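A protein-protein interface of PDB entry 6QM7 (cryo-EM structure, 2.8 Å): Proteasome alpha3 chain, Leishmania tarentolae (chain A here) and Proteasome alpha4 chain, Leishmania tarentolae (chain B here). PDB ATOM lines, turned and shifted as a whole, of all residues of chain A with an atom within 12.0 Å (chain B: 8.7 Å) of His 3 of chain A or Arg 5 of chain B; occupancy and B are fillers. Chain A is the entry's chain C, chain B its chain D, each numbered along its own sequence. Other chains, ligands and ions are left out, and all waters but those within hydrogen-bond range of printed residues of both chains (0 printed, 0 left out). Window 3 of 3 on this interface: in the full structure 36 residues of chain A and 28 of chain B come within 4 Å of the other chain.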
ATOM      1  N   SER A   2      21.167  28.460  16.384  1.00  0.00           N
ATOM      2  CA  SER A   2      19.746  28.212  16.786  1.00  0.00           C
ATOM      3  C   SER A   2      19.073  27.251  15.791  1.00  0.00           C
ATOM      4  O   SER A   2      18.304  26.408  16.263  1.00  0.00           O
ATOM      5  CB  SER A   2      18.965  29.510  16.959  1.00  0.00           C
ATOM      6  OG  SER A   2      18.052  29.451  18.050  1.00  0.00           O
ATOM      7  N   HIS A   3      19.369  27.312  14.486  1.00  0.00           N
ATOM      8  CA  HIS A   3      18.834  26.343  13.485  1.00  0.00           C
ATOM      9  C   HIS A   3      19.266  24.919  13.869  1.00  0.00           C
ATOM     10  O   HIS A   3      18.530  23.982  13.542  1.00  0.00           O
ATOM     11  CB  HIS A   3      19.226  26.716  12.039  1.00  0.00           C
ATOM     12  CG  HIS A   3      20.565  26.214  11.594  1.00  0.00           C
ATOM     13  ND1 HIS A   3      21.724  26.964  11.728  1.00  0.00           N
ATOM     14  CD2 HIS A   3      20.937  25.051  11.011  1.00  0.00           C
ATOM     15  CE1 HIS A   3      22.750  26.280  11.256  1.00  0.00           C
ATOM     16  NE2 HIS A   3      22.292  25.100  10.811  1.00  0.00           N
ATOM     17  N   ARG A   4      20.415  24.779  14.540  1.00  0.00           N
ATOM     18  CA  ARG A   4      21.013  23.491  14.995  1.00  0.00           C
ATOM     19  C   ARG A   4      20.034  22.738  15.900  1.00  0.00           C
ATOM     20  O   ARG A   4      20.000  21.504  15.819  1.00  0.00           O
ATOM     21  CB  ARG A   4      22.323  23.733  15.759  1.00  0.00           C
ATOM     22  CG  ARG A   4      23.444  24.366  14.936  1.00  0.00           C
ATOM     23  CD  ARG A   4      24.787  24.457  15.656  1.00  0.00           C
ATOM     24  NE  ARG A   4      25.242  23.143  16.125  1.00  0.00           N
ATOM     25  CZ  ARG A   4      25.411  22.756  17.399  1.00  0.00           C
ATOM     26  NH1 ARG A   4      25.815  21.520  17.654  1.00  0.00           N
ATOM     27  NH2 ARG A   4      25.201  23.580  18.415  1.00  0.00           N
ATOM     28  N   TYR A   5      19.278  23.465  16.727  1.00  0.00           N
ATOM     29  CA  TYR A   5      18.430  22.926  17.823  1.00  0.00           C
ATOM     30  C   TYR A   5      16.950  22.890  17.415  1.00  0.00           C
ATOM     31  O   TYR A   5      16.091  22.661  18.298  1.00  0.00           O
ATOM     32  CB  TYR A   5      18.611  23.757  19.099  1.00  0.00           C
ATOM     33  CG  TYR A   5      20.041  24.112  19.436  1.00  0.00           C
ATOM     34  CD1 TYR A   5      20.957  23.135  19.805  1.00  0.00           C
ATOM     35  CD2 TYR A   5      20.482  25.429  19.375  1.00  0.00           C
ATOM     36  CE1 TYR A   5      22.270  23.461  20.104  1.00  0.00           C
ATOM     37  CE2 TYR A   5      21.791  25.771  19.673  1.00  0.00           C
ATOM     38  CZ  TYR A   5      22.687  24.782  20.042  1.00  0.00           C
ATOM     39  OH  TYR A   5      23.979  25.116  20.331  1.00  0.00           O
ATOM     40  N   ASP A   6      16.650  23.100  16.129  1.00  0.00           N
ATOM     41  CA  ASP A   6      15.292  22.929  15.559  1.00  0.00           C
ATOM     42  C   ASP A   6      14.985  21.430  15.524  1.00  0.00           C
ATOM     43  O   ASP A   6      15.797  20.661  14.975  1.00  0.00           O
ATOM     44  CB  ASP A   6      15.182  23.572  14.174  1.00  0.00           C
ATOM     45  CG  ASP A   6      13.768  23.785  13.656  1.00  0.00           C
ATOM     46  OD1 ASP A   6      12.825  23.185  14.215  1.00  0.00           O
ATOM     47  OD2 ASP A   6      13.624  24.551  12.688  1.00  0.00           O
ATOM     48  N   SER A   7      13.847  21.056  16.108  1.00  0.00           N
ATOM     49  CA  SER A   7      13.292  19.678  16.182  1.00  0.00           C
ATOM     50  C   SER A   7      12.688  19.258  14.836  1.00  0.00           C
ATOM     51  O   SER A   7      12.542  18.037  14.615  1.00  0.00           O
ATOM     52  CB  SER A   7      12.260  19.634  17.266  1.00  0.00           C
ATOM     53  OG  SER A   7      11.532  20.859  17.275  1.00  0.00           O
ATOM     54  N   ARG A   8      12.318  20.241  14.002  1.00  0.00           N
ATOM     55  CA  ARG A   8      11.703  20.067  12.660  1.00  0.00           C
ATOM     56  C   ARG A   8      10.407  19.269  12.841  1.00  0.00           C
ATOM     57  O   ARG A   8      10.348  18.098  12.424  1.00  0.00           O
ATOM     58  CB  ARG A   8      12.733  19.467  11.692  1.00  0.00           C
ATOM     59  CG  ARG A   8      13.508  20.494  10.866  1.00  0.00           C
ATOM     60  CD  ARG A   8      15.021  20.339  10.922  1.00  0.00           C
ATOM     61  NE  ARG A   8      15.451  18.939  10.918  1.00  0.00           N
ATOM     62  CZ  ARG A   8      16.546  18.450  11.512  1.00  0.00           C
ATOM     63  NH1 ARG A   8      17.376  19.233  12.186  1.00  0.00           N
ATOM     64  NH2 ARG A   8      16.803  17.152  11.429  1.00  0.00           N
ATOM     65  N   THR A   9       9.420  19.899  13.481  1.00  0.00           N
ATOM     66  CA  THR A   9       8.121  19.292  13.866  1.00  0.00           C
ATOM     67  C   THR A   9       7.324  19.028  12.589  1.00  0.00           C
ATOM     68  O   THR A   9       6.836  17.898  12.432  1.00  0.00           O
ATOM     69  CB  THR A   9       7.342  20.168  14.868  1.00  0.00           C
ATOM     70  OG1 THR A   9       7.009  21.444  14.318  1.00  0.00           O
ATOM     71  CG2 THR A   9       8.099  20.416  16.154  1.00  0.00           C
ATOM     72  N   THR A  10       7.229  20.037  11.718  1.00  0.00           N
ATOM     73  CA  THR A  10       6.378  20.061  10.495  1.00  0.00           C
ATOM     74  C   THR A  10       7.205  19.580   9.297  1.00  0.00           C
ATOM     75  O   THR A  10       7.321  20.330   8.304  1.00  0.00           O
ATOM     76  CB  THR A  10       5.798  21.462  10.251  1.00  0.00           C
ATOM     77  OG1 THR A  10       6.842  22.389   9.937  1.00  0.00           O
ATOM     78  CG2 THR A  10       5.022  21.978  11.443  1.00  0.00           C
ATOM     79  N   THR A  11       7.796  18.395   9.417  1.00  0.00           N
ATOM     80  CA  THR A  11       8.531  17.716   8.332  1.00  0.00           C
ATOM     81  C   THR A  11       8.014  16.290   8.230  1.00  0.00           C
ATOM     82  O   THR A  11       7.628  15.724   9.256  1.00  0.00           O
ATOM     83  CB  THR A  11      10.044  17.668   8.575  1.00  0.00           C
ATOM     84  OG1 THR A  11      10.245  17.000   9.821  1.00  0.00           O
ATOM     85  CG2 THR A  11      10.683  19.038   8.577  1.00  0.00           C
ATOM     86  N   PHE A  12       8.041  15.745   7.026  1.00  0.00           N
ATOM     87  CA  PHE A  12       7.892  14.300   6.791  1.00  0.00           C
ATOM     88  C   PHE A  12       9.171  13.602   7.240  1.00  0.00           C
ATOM     89  O   PHE A  12      10.243  14.225   7.265  1.00  0.00           O
ATOM     90  CB  PHE A  12       7.614  14.036   5.317  1.00  0.00           C
ATOM     91  CG  PHE A  12       6.233  14.436   4.883  1.00  0.00           C
ATOM     92  CD1 PHE A  12       5.146  13.640   5.212  1.00  0.00           C
ATOM     93  CD2 PHE A  12       6.027  15.579   4.138  1.00  0.00           C
ATOM     94  CE1 PHE A  12       3.870  13.984   4.807  1.00  0.00           C
ATOM     95  CE2 PHE A  12       4.750  15.922   3.733  1.00  0.00           C
ATOM     96  CZ  PHE A  12       3.675  15.126   4.066  1.00  0.00           C
ATOM     97  N   GLN A 129       1.807  21.367   9.476  1.00  0.00           N
ATOM     98  CA  GLN A 129       2.334  21.780   8.144  1.00  0.00           C
ATOM     99  C   GLN A 129       3.176  23.060   8.255  1.00  0.00           C
ATOM    100  O   GLN A 129       4.296  23.051   7.742  1.00  0.00           O
ATOM    101  CB  GLN A 129       1.191  21.926   7.138  1.00  0.00           C
ATOM    102  CG  GLN A 129       1.655  21.816   5.689  1.00  0.00           C
ATOM    103  CD  GLN A 129       0.533  21.792   4.682  1.00  0.00           C
ATOM    104  OE1 GLN A 129      -0.647  21.861   5.021  1.00  0.00           O
ATOM    105  NE2 GLN A 129       0.903  21.700   3.416  1.00  0.00           N
ATOM    106  N   TYR A 130       2.654  24.113   8.889  1.00  0.00           N
ATOM    107  CA  TYR A 130       3.305  25.437   9.059  1.00  0.00           C
ATOM    108  C   TYR A 130       3.804  25.579  10.496  1.00  0.00           C
ATOM    109  O   TYR A 130       3.261  24.915  11.384  1.00  0.00           O
ATOM    110  CB  TYR A 130       2.311  26.551   8.704  1.00  0.00           C
ATOM    111  CG  TYR A 130       1.747  26.421   7.311  1.00  0.00           C
ATOM    112  CD1 TYR A 130       0.648  25.613   7.051  1.00  0.00           C
ATOM    113  CD2 TYR A 130       2.347  27.059   6.232  1.00  0.00           C
ATOM    114  CE1 TYR A 130       0.154  25.451   5.762  1.00  0.00           C
ATOM    115  CE2 TYR A 130       1.861  26.917   4.937  1.00  0.00           C
ATOM    116  CZ  TYR A 130       0.763  26.105   4.700  1.00  0.00           C
ATOM    117  OH  TYR A 130       0.285  25.957   3.430  1.00  0.00           O
ATOM    118  N   GLY A 131       4.826  26.415  10.707  1.00  0.00           N
ATOM    119  CA  GLY A 131       5.037  27.158  11.970  1.00  0.00           C
ATOM    120  C   GLY A 131       6.082  26.555  12.894  1.00  0.00           C
ATOM    121  O   GLY A 131       6.384  27.209  13.910  1.00  0.00           O
ATOM    122  N   GLY A 132       6.581  25.353  12.589  1.00  0.00           N
ATOM    123  CA  GLY A 132       7.711  24.713  13.287  1.00  0.00           C
ATOM    124  C   GLY A 132       7.489  24.515  14.776  1.00  0.00           C
ATOM    125  O   GLY A 132       8.496  24.412  15.508  1.00  0.00           O
ATOM    126  N   VAL A 133       6.235  24.395  15.203  1.00  0.00           N
ATOM    127  CA  VAL A 133       5.843  24.124  16.619  1.00  0.00           C
ATOM    128  C   VAL A 133       5.144  22.771  16.652  1.00  0.00           C
ATOM    129  O   VAL A 133       4.752  22.296  15.581  1.00  0.00           O
ATOM    130  CB  VAL A 133       4.947  25.232  17.196  1.00  0.00           C
ATOM    131  CG1 VAL A 133       5.751  26.494  17.425  1.00  0.00           C
ATOM    132  CG2 VAL A 133       3.735  25.532  16.325  1.00  0.00           C
ATOM    133  N   SER B   2       7.768  35.324  11.273  1.00  0.00           N
ATOM    134  CA  SER B   2       7.262  33.919  11.380  1.00  0.00           C
ATOM    135  C   SER B   2       8.399  32.933  11.085  1.00  0.00           C
ATOM    136  O   SER B   2       9.485  33.372  10.644  1.00  0.00           O
ATOM    137  CB  SER B   2       6.066  33.677  10.472  1.00  0.00           C
ATOM    138  OG  SER B   2       6.470  33.384   9.139  1.00  0.00           O
ATOM    139  N   TYR B   3       8.139  31.647  11.331  1.00  0.00           N
ATOM    140  CA  TYR B   3       9.072  30.521  11.082  1.00  0.00           C
ATOM    141  C   TYR B   3       9.110  30.247   9.583  1.00  0.00           C
ATOM    142  O   TYR B   3       8.123  29.682   9.067  1.00  0.00           O
ATOM    143  CB  TYR B   3       8.617  29.283  11.844  1.00  0.00           C
ATOM    144  CG  TYR B   3       9.388  28.014  11.593  1.00  0.00           C
ATOM    145  CD1 TYR B   3      10.605  27.778  12.203  1.00  0.00           C
ATOM    146  CD2 TYR B   3       8.851  27.004  10.817  1.00  0.00           C
ATOM    147  CE1 TYR B   3      11.285  26.584  12.016  1.00  0.00           C
ATOM    148  CE2 TYR B   3       9.522  25.807  10.612  1.00  0.00           C
ATOM    149  CZ  TYR B   3      10.746  25.590  11.216  1.00  0.00           C
ATOM    150  OH  TYR B   3      11.391  24.405  10.997  1.00  0.00           O
ATOM    151  N   ASP B   4      10.202  30.659   8.930  1.00  0.00           N
ATOM    152  CA  ASP B   4      10.458  30.442   7.485  1.00  0.00           C
ATOM    153  C   ASP B   4      11.791  29.711   7.321  1.00  0.00           C
ATOM    154  O   ASP B   4      12.539  30.068   6.404  1.00  0.00           O
ATOM    155  CB  ASP B   4      10.370  31.757   6.695  1.00  0.00           C
ATOM    156  CG  ASP B   4      11.289  32.903   7.120  1.00  0.00           C
ATOM    157  OD1 ASP B   4      12.374  32.636   7.686  1.00  0.00           O
ATOM    158  OD2 ASP B   4      10.918  34.071   6.862  1.00  0.00           O
ATOM    159  N   ARG B   5      12.064  28.703   8.149  1.00  0.00           N
ATOM    160  CA  ARG B   5      13.208  27.782   7.923  1.00  0.00           C
ATOM    161  C   ARG B   5      12.937  27.031   6.616  1.00  0.00           C
ATOM    162  O   ARG B   5      11.759  26.800   6.311  1.00  0.00           O
ATOM    163  CB  ARG B   5      13.396  26.824   9.104  1.00  0.00           C
ATOM    164  CG  ARG B   5      14.729  26.080   9.128  1.00  0.00           C
ATOM    165  CD  ARG B   5      14.565  24.565   9.223  1.00  0.00           C
ATOM    166  NE  ARG B   5      15.476  23.924  10.174  1.00  0.00           N
ATOM    167  CZ  ARG B   5      16.729  23.525   9.930  1.00  0.00           C
ATOM    168  NH1 ARG B   5      17.285  23.698   8.740  1.00  0.00           N
ATOM    169  NH2 ARG B   5      17.433  22.955  10.895  1.00  0.00           N
ATOM    170  N   ALA B   6      13.987  26.684   5.870  1.00  0.00           N
ATOM    171  CA  ALA B   6      13.904  25.878   4.627  1.00  0.00           C
ATOM    172  C   ALA B   6      13.708  24.409   4.999  1.00  0.00           C
ATOM    173  O   ALA B   6      14.620  23.847   5.617  1.00  0.00           O
ATOM    174  CB  ALA B   6      15.148  26.061   3.793  1.00  0.00           C
ATOM    175  N   ILE B   7      12.560  23.829   4.629  1.00  0.00           N
ATOM    176  CA  ILE B   7      12.170  22.424   4.962  1.00  0.00           C
ATOM    177  C   ILE B   7      12.410  21.521   3.746  1.00  0.00           C
ATOM    178  O   ILE B   7      12.982  20.437   3.917  1.00  0.00           O
ATOM    179  CB  ILE B   7      10.716  22.393   5.469  1.00  0.00           C
ATOM    180  CG1 ILE B   7      10.652  22.809   6.940  1.00  0.00           C
ATOM    181  CG2 ILE B   7      10.058  21.039   5.254  1.00  0.00           C
ATOM    182  CD1 ILE B   7       9.425  23.608   7.289  1.00  0.00           C
ATOM    183  N   THR B   8      11.949  21.946   2.573  1.00  0.00           N
ATOM    184  CA  THR B   8      12.155  21.233   1.290  1.00  0.00           C
ATOM    185  C   THR B   8      13.456  21.747   0.670  1.00  0.00           C
ATOM    186  O   THR B   8      13.490  22.930   0.250  1.00  0.00           O
ATOM    187  CB  THR B   8      10.952  21.407   0.356  1.00  0.00           C
ATOM    188  OG1 THR B   8       9.731  21.273   1.089  1.00  0.00           O
ATOM    189  CG2 THR B   8      10.987  20.406  -0.776  1.00  0.00           C
ATOM    190  N   VAL B   9      14.492  20.906   0.650  1.00  0.00           N
ATOM    191  CA  VAL B   9      15.863  21.287   0.197  1.00  0.00           C
ATOM    192  C   VAL B   9      16.463  20.136  -0.595  1.00  0.00           C
ATOM    193  O   VAL B   9      16.104  18.985  -0.327  1.00  0.00           O
ATOM    194  CB  VAL B   9      16.768  21.659   1.384  1.00  0.00           C
ATOM    195  CG1 VAL B   9      16.153  22.786   2.204  1.00  0.00           C
ATOM    196  CG2 VAL B   9      17.099  20.450   2.252  1.00  0.00           C
ATOM    197  N   GLN B 120       8.396  24.669  -1.962  1.00  0.00           N
ATOM    198  CA  GLN B 120       9.396  25.768  -2.079  1.00  0.00           C
ATOM    199  C   GLN B 120       9.155  26.881  -1.042  1.00  0.00           C
ATOM    200  O   GLN B 120      10.037  27.740  -0.891  1.00  0.00           O
ATOM    201  CB  GLN B 120       9.367  26.319  -3.508  1.00  0.00           C
ATOM    202  CG  GLN B 120      10.734  26.732  -4.034  1.00  0.00           C
ATOM    203  CD  GLN B 120      10.696  27.131  -5.486  1.00  0.00           C
ATOM    204  OE1 GLN B 120       9.628  27.366  -6.054  1.00  0.00           O
ATOM    205  NE2 GLN B 120      11.872  27.197  -6.100  1.00  0.00           N
ATOM    206  N   SER B 121       8.007  26.894  -0.366  1.00  0.00           N
ATOM    207  CA  SER B 121       7.722  27.792   0.779  1.00  0.00           C
ATOM    208  C   SER B 121       8.599  27.372   1.958  1.00  0.00           C
ATOM    209  O   SER B 121       8.546  26.187   2.359  1.00  0.00           O
ATOM    210  CB  SER B 121       6.258  27.767   1.150  1.00  0.00           C
ATOM    211  OG  SER B 121       5.962  28.766   2.118  1.00  0.00           O
ATOM    212  N   GLY B 122       9.415  28.304   2.446  1.00  0.00           N
ATOM    213  CA  GLY B 122      10.085  28.179   3.746  1.00  0.00           C
ATOM    214  C   GLY B 122       9.046  28.181   4.846  1.00  0.00           C
ATOM    215  O   GLY B 122       8.184  29.087   4.820  1.00  0.00           O
ATOM    216  N   GLY B 123       9.116  27.201   5.753  1.00  0.00           N
ATOM    217  CA  GLY B 123       8.272  27.108   6.958  1.00  0.00           C
ATOM    218  C   GLY B 123       7.258  25.982   6.859  1.00  0.00           C
ATOM    219  O   GLY B 123       6.659  25.620   7.907  1.00  0.00           O
ATOM    220  N   SER B 124       7.091  25.416   5.662  1.00  0.00           N
ATOM    221  CA  SER B 124       6.030  24.429   5.352  1.00  0.00           C
ATOM    222  C   SER B 124       6.669  23.167   4.789  1.00  0.00           C
ATOM    223  O   SER B 124       7.649  23.280   4.030  1.00  0.00           O
ATOM    224  CB  SER B 124       5.001  24.992   4.393  1.00  0.00           C
ATOM    225  OG  SER B 124       4.904  26.406   4.516  1.00  0.00           O
ATOM    226  N   ARG B 125       6.104  22.015   5.145  1.00  0.00           N
ATOM    227  CA  ARG B 125       6.342  20.755   4.406  1.00  0.00           C
ATOM    228  C   ARG B 125       5.421  20.776   3.196  1.00  0.00           C
ATOM    229  O   ARG B 125       4.459  21.551   3.161  1.00  0.00           O
ATOM    230  CB  ARG B 125       6.091  19.508   5.259  1.00  0.00           C
ATOM    231  CG  ARG B 125       4.694  19.424   5.843  1.00  0.00           C
ATOM    232  CD  ARG B 125       4.462  18.103   6.526  1.00  0.00           C
ATOM    233  NE  ARG B 125       3.149  18.144   7.148  1.00  0.00           N
ATOM    234  CZ  ARG B 125       1.994  18.026   6.502  1.00  0.00           C
ATOM    235  NH1 ARG B 125       1.967  17.822   5.191  1.00  0.00           N
ATOM    236  NH2 ARG B 125       0.863  18.102   7.185  1.00  0.00           N
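Among the printed residues, merely in contact across the chains: Arg 8 of chain A with Arg 5 of chain B, Thr 10 of chain A with Ile 7 of chain B, Thr 10 of chain A with Gly 123 of chain B, Thr 10 of chain A with Arg 125 of chain B, Thr 11 of chain A with Ile 7 of chain B, Phe 12 of chain A with Arg 125 of chain B, Gln 129 of chain A with Ser 124 of chain B, Tyr 130 of chain A with Gly 123 of chain B, Tyr 130 of chain A with Ser 124 of chain B, Gly 131 of chain A with Tyr 3 of chain B and Gly 132 of chain A with Tyr 3 of chain B.
Printed residues of chain B within 4 Å of His 3 of chain A: Arg 5.
Arg 5 of chain B touches just these residues of chain A: His 3, Asp 6 and Arg 8.
No residue of chain B comes within 4 Å of Ser 2 of chain A.
No residue of chain A comes within 4 Å of Ala 6 of chain B.
Ile 7 of chain B touches two residues of chain A.
Of chain A, only Gln 129 (3.3 Å) and Tyr 130 (3.1 Å) come within 4 Å of Ser 124 of chain B.
Printed residues of chain A within 4 Å of Arg 125 of chain B: Thr 10, Phe 12 and Gln 129.
Of the printed residues of chain B, Arg 8 of chain A touches Arg 5.
Of the printed residues of chain B, Thr 11 of chain A touches Ile 7 (3.9 Å).
Ser 7 of chain A touches none of the printed residues of chain B.
The nearest residue of chain B that does not touch His 3 of chain A is Tyr 3 of chain B (7.6 Å).
The nearest residue of chain A that does not touch Arg 5 of chain B is Arg 4 of chain A (5.1 Å).
The backbone NH (N) of Arg 8 of chain A sits at hydrogen-bond distance from the side-chain carboxylate (OD1) of Asp 6 of chain A, 3.0 Å away.
O of Arg 8 of chain A sits at hydrogen-bond distance from OG1 of Thr 11 of chain A (2.8 Å).
The side-chain hydroxyl of Thr 10 of chain A lies close to the backbone carbonyl oxygen of Gln 129 of chain A (3.4 Å).
O of Arg 5 of chain B sits at hydrogen-bond distance from N of Gly 123 of chain B (2.7 Å).
O of His 3 of chain A is in hydrogen-bond range of NH2 of Arg 5 of chain B (3.0 Å).
The side-chain carboxylate of Asp 6 of chain A sits at hydrogen-bond distance from the side-chain hydroxyl of Tyr 3 of chain B, 2.8 Å away.
The side-chain carboxylate (OD2) of Asp 6 of chain A is in salt-bridge range of the guanidinium group (NE) of Arg 5 of chain B (3.2 Å).
The backbone NH of Arg 125 of chain B sits at hydrogen-bond distance from the backbone carbonyl oxygen of Gln 129 of chain A (3.3 Å).
O of Gly 123 of chain B lies within hydrogen-bond range of N of Gly 131 of chain A.
O of Gly 123 of chain B lies close to O of Gln 129 of chain A, 3.5 Å away.
Hydrophobic or aromatic side chains of chain B within 4 Å of the printed part of chain A: Tyr 3 and Ile 7.
Printed residues of chain A that touch a printed residue of chain B: His 3, Asp 6, Arg 8, Thr 10, Thr 11, Phe 12, Gln 129, Tyr 130, Gly 131 and Gly 132.
Among the printed residues, Asp or Glu carboxylates within 4 Å of a Lys or Arg side-chain nitrogen of the other chain: Asp 6 of chain A with Arg 5 of chain B.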
